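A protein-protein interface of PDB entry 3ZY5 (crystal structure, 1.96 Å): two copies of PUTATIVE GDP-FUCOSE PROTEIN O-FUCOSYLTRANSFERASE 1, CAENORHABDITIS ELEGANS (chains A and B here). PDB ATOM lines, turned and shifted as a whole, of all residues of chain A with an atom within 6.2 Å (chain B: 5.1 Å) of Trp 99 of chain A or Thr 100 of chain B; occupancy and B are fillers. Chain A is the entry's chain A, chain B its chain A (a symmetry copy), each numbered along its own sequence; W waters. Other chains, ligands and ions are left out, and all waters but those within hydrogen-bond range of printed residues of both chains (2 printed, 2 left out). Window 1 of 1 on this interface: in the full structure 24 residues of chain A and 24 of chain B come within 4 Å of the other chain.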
ATOM      1  N   PHE A  97      15.859 -24.357   9.316  1.00  0.00           N
ATOM      2  CA  PHE A  97      16.237 -24.356  10.742  1.00  0.00           C
ATOM      3  C   PHE A  97      17.758 -24.281  10.887  1.00  0.00           C
ATOM      4  O   PHE A  97      18.504 -25.040  10.248  1.00  0.00           O
ATOM      5  CB  PHE A  97      15.723 -25.603  11.459  1.00  0.00           C
ATOM      6  CG  PHE A  97      14.221 -25.626  11.695  1.00  0.00           C
ATOM      7  CD1 PHE A  97      13.330 -25.760  10.622  1.00  0.00           C
ATOM      8  CD2 PHE A  97      13.710 -25.570  12.989  1.00  0.00           C
ATOM      9  CE1 PHE A  97      11.951 -25.820  10.831  1.00  0.00           C
ATOM     10  CE2 PHE A  97      12.329 -25.607  13.215  1.00  0.00           C
ATOM     11  CZ  PHE A  97      11.443 -25.737  12.117  1.00  0.00           C
ATOM     12  N   CYS A  98      18.212 -23.332  11.705  1.00  0.00           N
ATOM     13  CA  CYS A  98      19.612 -23.182  12.010  1.00  0.00           C
ATOM     14  C   CYS A  98      19.794 -22.611  13.400  1.00  0.00           C
ATOM     15  O   CYS A  98      18.815 -22.288  14.086  1.00  0.00           O
ATOM     16  CB  CYS A  98      20.342 -22.330  10.945  1.00  0.00           C
ATOM     17  SG  CYS A  98      19.777 -20.607  10.807  1.00  0.00           S
ATOM     18  N   TRP A  99      21.045 -22.480  13.826  1.00  0.00           N
ATOM     19  CA  TRP A  99      21.312 -22.003  15.196  1.00  0.00           C
ATOM     20  C   TRP A  99      20.868 -20.547  15.424  1.00  0.00           C
ATOM     21  O   TRP A  99      20.262 -20.213  16.457  1.00  0.00           O
ATOM     22  CB  TRP A  99      22.819 -22.127  15.531  1.00  0.00           C
ATOM     23  CG  TRP A  99      23.327 -23.561  15.757  1.00  0.00           C
ATOM     24  CD1 TRP A  99      23.727 -24.436  14.804  1.00  0.00           C
ATOM     25  CD2 TRP A  99      23.478 -24.248  17.015  1.00  0.00           C
ATOM     26  NE1 TRP A  99      24.138 -25.606  15.357  1.00  0.00           N
ATOM     27  CE2 TRP A  99      23.991 -25.533  16.721  1.00  0.00           C
ATOM     28  CE3 TRP A  99      23.225 -23.907  18.350  1.00  0.00           C
ATOM     29  CZ2 TRP A  99      24.266 -26.487  17.709  1.00  0.00           C
ATOM     30  CZ3 TRP A  99      23.515 -24.873  19.370  1.00  0.00           C
ATOM     31  CH2 TRP A  99      24.025 -26.141  19.030  1.00  0.00           C
ATOM     32  N   THR A 100      21.171 -19.669  14.467  1.00  0.00           N
ATOM     33  CA  THR A 100      21.087 -18.237  14.711  1.00  0.00           C
ATOM     34  C   THR A 100      21.076 -17.534  13.335  1.00  0.00           C
ATOM     35  O   THR A 100      21.477 -18.141  12.345  1.00  0.00           O
ATOM     36  CB  THR A 100      22.292 -17.779  15.598  1.00  0.00           C
ATOM     37  OG1 THR A 100      21.971 -16.581  16.321  1.00  0.00           O
ATOM     38  CG2 THR A 100      23.590 -17.589  14.773  1.00  0.00           C
ATOM     39  N   PRO A 101      20.519 -16.309  13.260  1.00  0.00           N
ATOM     40  CA  PRO A 101      20.597 -15.577  11.999  1.00  0.00           C
ATOM     41  C   PRO A 101      22.041 -15.126  11.690  1.00  0.00           C
ATOM     42  O   PRO A 101      22.798 -14.718  12.599  1.00  0.00           O
ATOM     43  CB  PRO A 101      19.681 -14.374  12.237  1.00  0.00           C
ATOM     44  CG  PRO A 101      19.633 -14.242  13.783  1.00  0.00           C
ATOM     45  CD  PRO A 101      19.614 -15.651  14.231  1.00  0.00           C
ATOM     46  N   CYS A 114      19.326 -18.018   8.028  1.00  0.00           N
ATOM     47  CA  CYS A 114      20.051 -19.275   7.858  1.00  0.00           C
ATOM     48  C   CYS A 114      20.768 -19.330   6.542  1.00  0.00           C
ATOM     49  O   CYS A 114      21.769 -20.062   6.405  1.00  0.00           O
ATOM     50  CB  CYS A 114      19.079 -20.474   7.917  1.00  0.00           C
ATOM     51  SG  CYS A 114      18.249 -20.661   9.534  1.00  0.00           S
ATOM     52  N   GLU A 137      13.761 -20.483  11.263  1.00  0.00           N
ATOM     53  CA  GLU A 137      13.530 -20.662  12.700  1.00  0.00           C
ATOM     54  C   GLU A 137      14.886 -21.026  13.263  1.00  0.00           C
ATOM     55  O   GLU A 137      15.705 -21.600  12.556  1.00  0.00           O
ATOM     56  CB  GLU A 137      12.570 -21.824  12.968  1.00  0.00           C
ATOM     57  CG  GLU A 137      11.229 -21.706  12.238  1.00  0.00           C
ATOM     58  CD  GLU A 137      10.275 -20.736  12.921  1.00  0.00           C
ATOM     59  OE1 GLU A 137      10.550 -20.293  14.066  1.00  0.00           O
ATOM     60  OE2 GLU A 137       9.231 -20.425  12.315  1.00  0.00           O
ATOM     61  N   TYR A 138      15.091 -20.733  14.546  1.00  0.00           N
ATOM     62  CA  TYR A 138      16.377 -20.860  15.178  1.00  0.00           C
ATOM     63  C   TYR A 138      16.223 -21.731  16.378  1.00  0.00           C
ATOM     64  O   TYR A 138      15.192 -21.667  17.071  1.00  0.00           O
ATOM     65  CB  TYR A 138      16.889 -19.466  15.600  1.00  0.00           C
ATOM     66  CG  TYR A 138      16.924 -18.492  14.430  1.00  0.00           C
ATOM     67  CD1 TYR A 138      17.729 -18.732  13.333  1.00  0.00           C
ATOM     68  CD2 TYR A 138      16.074 -17.370  14.404  1.00  0.00           C
ATOM     69  CE1 TYR A 138      17.718 -17.860  12.238  1.00  0.00           C
ATOM     70  CE2 TYR A 138      16.064 -16.507  13.333  1.00  0.00           C
ATOM     71  CZ  TYR A 138      16.892 -16.756  12.254  1.00  0.00           C
ATOM     72  OH  TYR A 138      16.896 -15.898  11.174  1.00  0.00           O
ATOM     73  N   PHE A 139      17.255 -22.531  16.657  1.00  0.00           N
ATOM     74  CA  PHE A 139      17.197 -23.426  17.828  1.00  0.00           C
ATOM     75  C   PHE A 139      18.293 -23.183  18.863  1.00  0.00           C
ATOM     76  O   PHE A 139      18.490 -24.005  19.775  1.00  0.00           O
ATOM     77  CB  PHE A 139      17.163 -24.906  17.399  1.00  0.00           C
ATOM     78  CG  PHE A 139      18.284 -25.302  16.457  1.00  0.00           C
ATOM     79  CD1 PHE A 139      19.551 -25.569  16.943  1.00  0.00           C
ATOM     80  CD2 PHE A 139      18.051 -25.392  15.068  1.00  0.00           C
ATOM     81  CE1 PHE A 139      20.623 -25.909  16.063  1.00  0.00           C
ATOM     82  CE2 PHE A 139      19.059 -25.743  14.196  1.00  0.00           C
ATOM     83  CZ  PHE A 139      20.377 -25.992  14.686  1.00  0.00           C
ATOM     84  N   GLY A 140      19.025 -22.075  18.720  1.00  0.00           N
ATOM     85  CA  GLY A 140      20.100 -21.736  19.660  1.00  0.00           C
ATOM     86  C   GLY A 140      19.660 -21.670  21.111  1.00  0.00           C
ATOM     87  O   GLY A 140      20.461 -21.961  22.014  1.00  0.00           O
ATOM     88  N   ASP A 141      18.397 -21.304  21.331  1.00  0.00           N
ATOM     89  CA  ASP A 141      17.879 -21.094  22.697  1.00  0.00           C
ATOM     90  C   ASP A 141      17.464 -22.414  23.397  1.00  0.00           C
ATOM     91  O   ASP A 141      17.239 -22.463  24.608  1.00  0.00           O
ATOM     92  CB  ASP A 141      16.787 -20.004  22.758  1.00  0.00           C
ATOM     93  CG  ASP A 141      15.517 -20.357  21.981  1.00  0.00           C
ATOM     94  OD1 ASP A 141      15.273 -21.539  21.675  1.00  0.00           O
ATOM     95  OD2 ASP A 141      14.740 -19.430  21.678  1.00  0.00           O
ATOM     96  N   ILE A 142      17.411 -23.477  22.611  1.00  0.00           N
ATOM     97  CA  ILE A 142      17.360 -24.836  23.150  1.00  0.00           C
ATOM     98  C   ILE A 142      18.753 -25.273  23.650  1.00  0.00           C
ATOM     99  O   ILE A 142      19.701 -25.284  22.887  1.00  0.00           O
ATOM    100  CB  ILE A 142      16.835 -25.801  22.077  1.00  0.00           C
ATOM    101  CG1 ILE A 142      15.465 -25.312  21.620  1.00  0.00           C
ATOM    102  CG2 ILE A 142      16.831 -27.258  22.616  1.00  0.00           C
ATOM    103  CD1 ILE A 142      14.917 -26.039  20.395  1.00  0.00           C
ATOM    104  N   GLY A 144      22.108 -26.658  24.111  1.00  0.00           N
ATOM    105  CA  GLY A 144      22.950 -27.552  23.302  1.00  0.00           C
ATOM    106  C   GLY A 144      22.466 -27.763  21.882  1.00  0.00           C
ATOM    107  O   GLY A 144      22.919 -28.697  21.196  1.00  0.00           O
ATOM    108  N   GLY A 145      21.558 -26.900  21.420  1.00  0.00           N
ATOM    109  CA  GLY A 145      20.989 -27.016  20.075  1.00  0.00           C
ATOM    110  C   GLY A 145      20.360 -28.367  19.788  1.00  0.00           C
ATOM    111  O   GLY A 145      19.345 -28.730  20.401  1.00  0.00           O
ATOM    112  N   PHE A 146      20.988 -29.138  18.886  1.00  0.00           N
ATOM    113  CA  PHE A 146      20.513 -30.482  18.534  1.00  0.00           C
ATOM    114  C   PHE A 146      21.142 -31.611  19.365  1.00  0.00           C
ATOM    115  O   PHE A 146      20.945 -32.793  19.081  1.00  0.00           O
ATOM    116  CB  PHE A 146      20.774 -30.741  17.053  1.00  0.00           C
ATOM    117  CG  PHE A 146      22.141 -30.321  16.604  1.00  0.00           C
ATOM    118  CD1 PHE A 146      23.297 -30.932  17.129  1.00  0.00           C
ATOM    119  CD2 PHE A 146      22.280 -29.293  15.677  1.00  0.00           C
ATOM    120  CE1 PHE A 146      24.579 -30.514  16.719  1.00  0.00           C
ATOM    121  CE2 PHE A 146      23.530 -28.895  15.231  1.00  0.00           C
ATOM    122  CZ  PHE A 146      24.698 -29.504  15.757  1.00  0.00           C
ATOM    123  N   ASP A 147      21.934 -31.262  20.371  1.00  0.00           N
ATOM    124  CA  ASP A 147      22.646 -32.296  21.125  1.00  0.00           C
ATOM    125  C   ASP A 147      21.748 -33.277  21.900  1.00  0.00           C
ATOM    126  O   ASP A 147      22.018 -34.487  21.910  1.00  0.00           O
ATOM    127  CB  ASP A 147      23.636 -31.665  22.079  1.00  0.00           C
ATOM    128  CG  ASP A 147      24.880 -31.193  21.404  1.00  0.00           C
ATOM    129  OD1 ASP A 147      25.060 -31.418  20.165  1.00  0.00           O
ATOM    130  OD2 ASP A 147      25.689 -30.585  22.136  1.00  0.00           O
ATOM    131  N   SER A 173      22.078 -27.455   7.727  1.00  0.00           N
ATOM    132  CA  SER A 173      23.202 -28.387   7.810  1.00  0.00           C
ATOM    133  C   SER A 173      22.826 -29.486   8.812  1.00  0.00           C
ATOM    134  O   SER A 173      21.885 -29.317   9.612  1.00  0.00           O
ATOM    135  CB  SER A 173      24.480 -27.667   8.229  1.00  0.00           C
ATOM    136  OG  SER A 173      24.365 -27.219   9.572  1.00  0.00           O
ATOM    137  N   ALA A 176      23.919 -32.389  13.926  1.00  0.00           N
ATOM    138  CA  ALA A 176      24.716 -33.379  14.632  1.00  0.00           C
ATOM    139  C   ALA A 176      26.113 -32.852  14.930  1.00  0.00           C
ATOM    140  O   ALA A 176      26.658 -32.069  14.123  1.00  0.00           O
ATOM    141  CB  ALA A 176      24.814 -34.658  13.799  1.00  0.00           C
ATOM    142  N   CYS B  98      32.352 -18.954  17.826  1.00  0.00           N
ATOM    143  CA  CYS B  98      31.078 -18.999  17.155  1.00  0.00           C
ATOM    144  C   CYS B  98      30.230 -20.127  17.703  1.00  0.00           C
ATOM    145  O   CYS B  98      30.676 -20.896  18.564  1.00  0.00           O
ATOM    146  CB  CYS B  98      31.241 -19.102  15.621  1.00  0.00           C
ATOM    147  SG  CYS B  98      32.058 -20.615  15.027  1.00  0.00           S
ATOM    148  N   TRP B  99      29.003 -20.238  17.207  1.00  0.00           N
ATOM    149  CA  TRP B  99      28.082 -21.262  17.737  1.00  0.00           C
ATOM    150  C   TRP B  99      28.549 -22.699  17.445  1.00  0.00           C
ATOM    151  O   TRP B  99      28.498 -23.582  18.319  1.00  0.00           O
ATOM    152  CB  TRP B  99      26.660 -21.067  17.156  1.00  0.00           C
ATOM    153  CG  TRP B  99      25.886 -19.856  17.703  1.00  0.00           C
ATOM    154  CD1 TRP B  99      25.966 -18.579  17.259  1.00  0.00           C
ATOM    155  CD2 TRP B  99      24.931 -19.842  18.783  1.00  0.00           C
ATOM    156  NE1 TRP B  99      25.127 -17.767  17.953  1.00  0.00           N
ATOM    157  CE2 TRP B  99      24.476 -18.508  18.910  1.00  0.00           C
ATOM    158  CE3 TRP B  99      24.426 -20.817  19.653  1.00  0.00           C
ATOM    159  CZ2 TRP B  99      23.532 -18.114  19.867  1.00  0.00           C
ATOM    160  CZ3 TRP B  99      23.451 -20.425  20.628  1.00  0.00           C
ATOM    161  CH2 TRP B  99      23.026 -19.085  20.718  1.00  0.00           C
ATOM    162  N   THR B 100      28.998 -22.948  16.214  1.00  0.00           N
ATOM    163  CA  THR B 100      29.161 -24.313  15.738  1.00  0.00           C
ATOM    164  C   THR B 100      30.073 -24.261  14.492  1.00  0.00           C
ATOM    165  O   THR B 100      30.218 -23.197  13.895  1.00  0.00           O
ATOM    166  CB  THR B 100      27.761 -24.935  15.419  1.00  0.00           C
ATOM    167  OG1 THR B 100      27.802 -26.367  15.510  1.00  0.00           O
ATOM    168  CG2 THR B 100      27.223 -24.490  14.036  1.00  0.00           C
ATOM    169  N   PRO B 101      30.766 -25.374  14.174  1.00  0.00           N
ATOM    170  CA  PRO B 101      31.546 -25.387  12.940  1.00  0.00           C
ATOM    171  C   PRO B 101      30.637 -25.390  11.691  1.00  0.00           C
ATOM    172  O   PRO B 101      29.576 -26.053  11.667  1.00  0.00           O
ATOM    173  CB  PRO B 101      32.344 -26.690  13.046  1.00  0.00           C
ATOM    174  CG  PRO B 101      31.519 -27.552  14.039  1.00  0.00           C
ATOM    175  CD  PRO B 101      31.045 -26.555  15.023  1.00  0.00           C
ATOM    176  N   ARG B 102      31.057 -24.669  10.653  1.00  0.00           N
ATOM    177  CA  ARG B 102      30.246 -24.563   9.439  1.00  0.00           C
ATOM    178  C   ARG B 102      31.107 -24.772   8.224  1.00  0.00           C
ATOM    179  O   ARG B 102      32.339 -24.639   8.295  1.00  0.00           O
ATOM    180  CB  ARG B 102      29.562 -23.187   9.360  1.00  0.00           C
ATOM    181  CG  ARG B 102      28.329 -23.116  10.286  1.00  0.00           C
ATOM    182  CD  ARG B 102      27.675 -21.735  10.324  1.00  0.00           C
ATOM    183  NE  ARG B 102      26.607 -21.569   9.327  1.00  0.00           N
ATOM    184  CZ  ARG B 102      26.787 -21.005   8.140  1.00  0.00           C
ATOM    185  NH1 ARG B 102      28.003 -20.593   7.786  1.00  0.00           N
ATOM    186  NH2 ARG B 102      25.763 -20.868   7.298  1.00  0.00           N
ATOM    187  N   GLY B 113      34.619 -24.841  10.456  1.00  0.00           N
ATOM    188  CA  GLY B 113      34.932 -23.821  11.460  1.00  0.00           C
ATOM    189  C   GLY B 113      34.012 -22.625  11.470  1.00  0.00           C
ATOM    190  O   GLY B 113      32.942 -22.645  10.852  1.00  0.00           O
ATOM    191  N   CYS B 114      34.438 -21.589  12.195  1.00  0.00           N
ATOM    192  CA  CYS B 114      33.746 -20.304  12.270  1.00  0.00           C
ATOM    193  C   CYS B 114      33.914 -19.509  11.010  1.00  0.00           C
ATOM    194  O   CYS B 114      33.068 -18.646  10.697  1.00  0.00           O
ATOM    195  CB  CYS B 114      34.294 -19.459  13.440  1.00  0.00           C
ATOM    196  SG  CYS B 114      34.005 -20.210  15.081  1.00  0.00           S
ATOM    197  N   TYR B 138      33.660 -23.071  20.258  1.00  0.00           N
ATOM    198  CA  TYR B 138      32.245 -23.052  20.002  1.00  0.00           C
ATOM    199  C   TYR B 138      31.538 -22.901  21.306  1.00  0.00           C
ATOM    200  O   TYR B 138      31.980 -23.458  22.327  1.00  0.00           O
ATOM    201  CB  TYR B 138      31.821 -24.371  19.322  1.00  0.00           C
ATOM    202  CG  TYR B 138      32.624 -24.644  18.057  1.00  0.00           C
ATOM    203  CD1 TYR B 138      32.565 -23.780  16.981  1.00  0.00           C
ATOM    204  CD2 TYR B 138      33.506 -25.739  17.988  1.00  0.00           C
ATOM    205  CE1 TYR B 138      33.345 -24.008  15.841  1.00  0.00           C
ATOM    206  CE2 TYR B 138      34.269 -25.972  16.868  1.00  0.00           C
ATOM    207  CZ  TYR B 138      34.182 -25.104  15.796  1.00  0.00           C
ATOM    208  OH  TYR B 138      34.937 -25.325  14.664  1.00  0.00           O
ATOM    209  N   GLY B 140      27.890 -23.266  21.425  1.00  0.00           N
ATOM    210  CA  GLY B 140      26.544 -23.831  21.272  1.00  0.00           C
ATOM    211  C   GLY B 140      26.078 -24.656  22.458  1.00  0.00           C
ATOM    212  O   GLY B 140      24.869 -24.706  22.740  1.00  0.00           O
HETATM  213  O   HOH W   1      26.937 -26.074  10.324  1.00  0.00           O
HETATM  214  O   HOH W   2      23.681 -22.266   5.382  1.00  0.00           O
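The backbone NH (N) of Gly 140 of chain A lies within hydrogen-bond range of the backbone carbonyl oxygen (O) of Trp 99 of chain A (3.2 Å).
N of Gly 140 of chain B lies within hydrogen-bond range of O of Trp 99 of chain B, 3.2 Å away.
The side-chain sulfur (SG) of Cys 98 of chain A forms a disulfide with the side-chain sulfur (SG) of Cys 114 of chain A (2.0 Å).
SG of Cys 114 of chain B forms a disulfide with SG of Cys 98 of chain B (2.0 Å).
Among the printed residues, pairs that only touch across the chains: Gly 144 of chain A with Gly 140 of chain B (3.5 Å), Thr 100 of chain A with Trp 99 of chain B (3.5 Å), Trp 99 of chain A with Thr 100 of chain B (3.5 Å), Trp 99 of chain A with Trp 99 of chain B (3.6 Å), Trp 99 of chain A with Gly 140 of chain B (3.6 Å) and Gly 140 of chain A with Trp 99 of chain B (3.6 Å).
Of the printed residues of chain A, Thr 100 of chain B touches Trp 99 (3.5 Å).
Of the printed residues of chain A, Gly 140 of chain B touches Trp 99 and Gly 144.
Of the printed residues of chain B, Gly 144 of chain A touches Gly 140.
Of the printed residues of chain B, Thr 100 of chain A touches Trp 99 (3.5 Å).
Of the 9 printed residues of chain B, 3 touch a printed residue of chain A.
Hydrophobic or aromatic side chains of chain B within 4 Å of the printed part of chain A: Trp 99.
Hydrophobic or aromatic side chains of chain A within 4 Å of the printed part of chain B: Trp 99.
Among the printed residues, 6 pairs touch across the chains.
Trp 99 of chain A touches its own counterpart, Trp 99 of chain B.
Trp 99 of chain A touches Thr 100 of chain B, and with the chains exchanged Thr 100 of chain A touches Trp 99 of chain B.
Trp 99 of chain A touches Gly 140 of chain B, and with the chains exchanged Gly 140 of chain A touches Trp 99 of chain B.
7 positions are printed for both chains.
Of the 6 pairs that touch across the chains among the printed residues, 5 have their exchanged pair printed and touching as well.
Water W1 lies within hydrogen-bond range of the side-chain hydroxyl of Ser 173 of chain A and the backbone carbonyl oxygen of Pro 101 of chain B.
Water W2 lies within hydrogen-bond range of O of Cys 114 of chain A and NH2 of Arg 102 of chain B.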
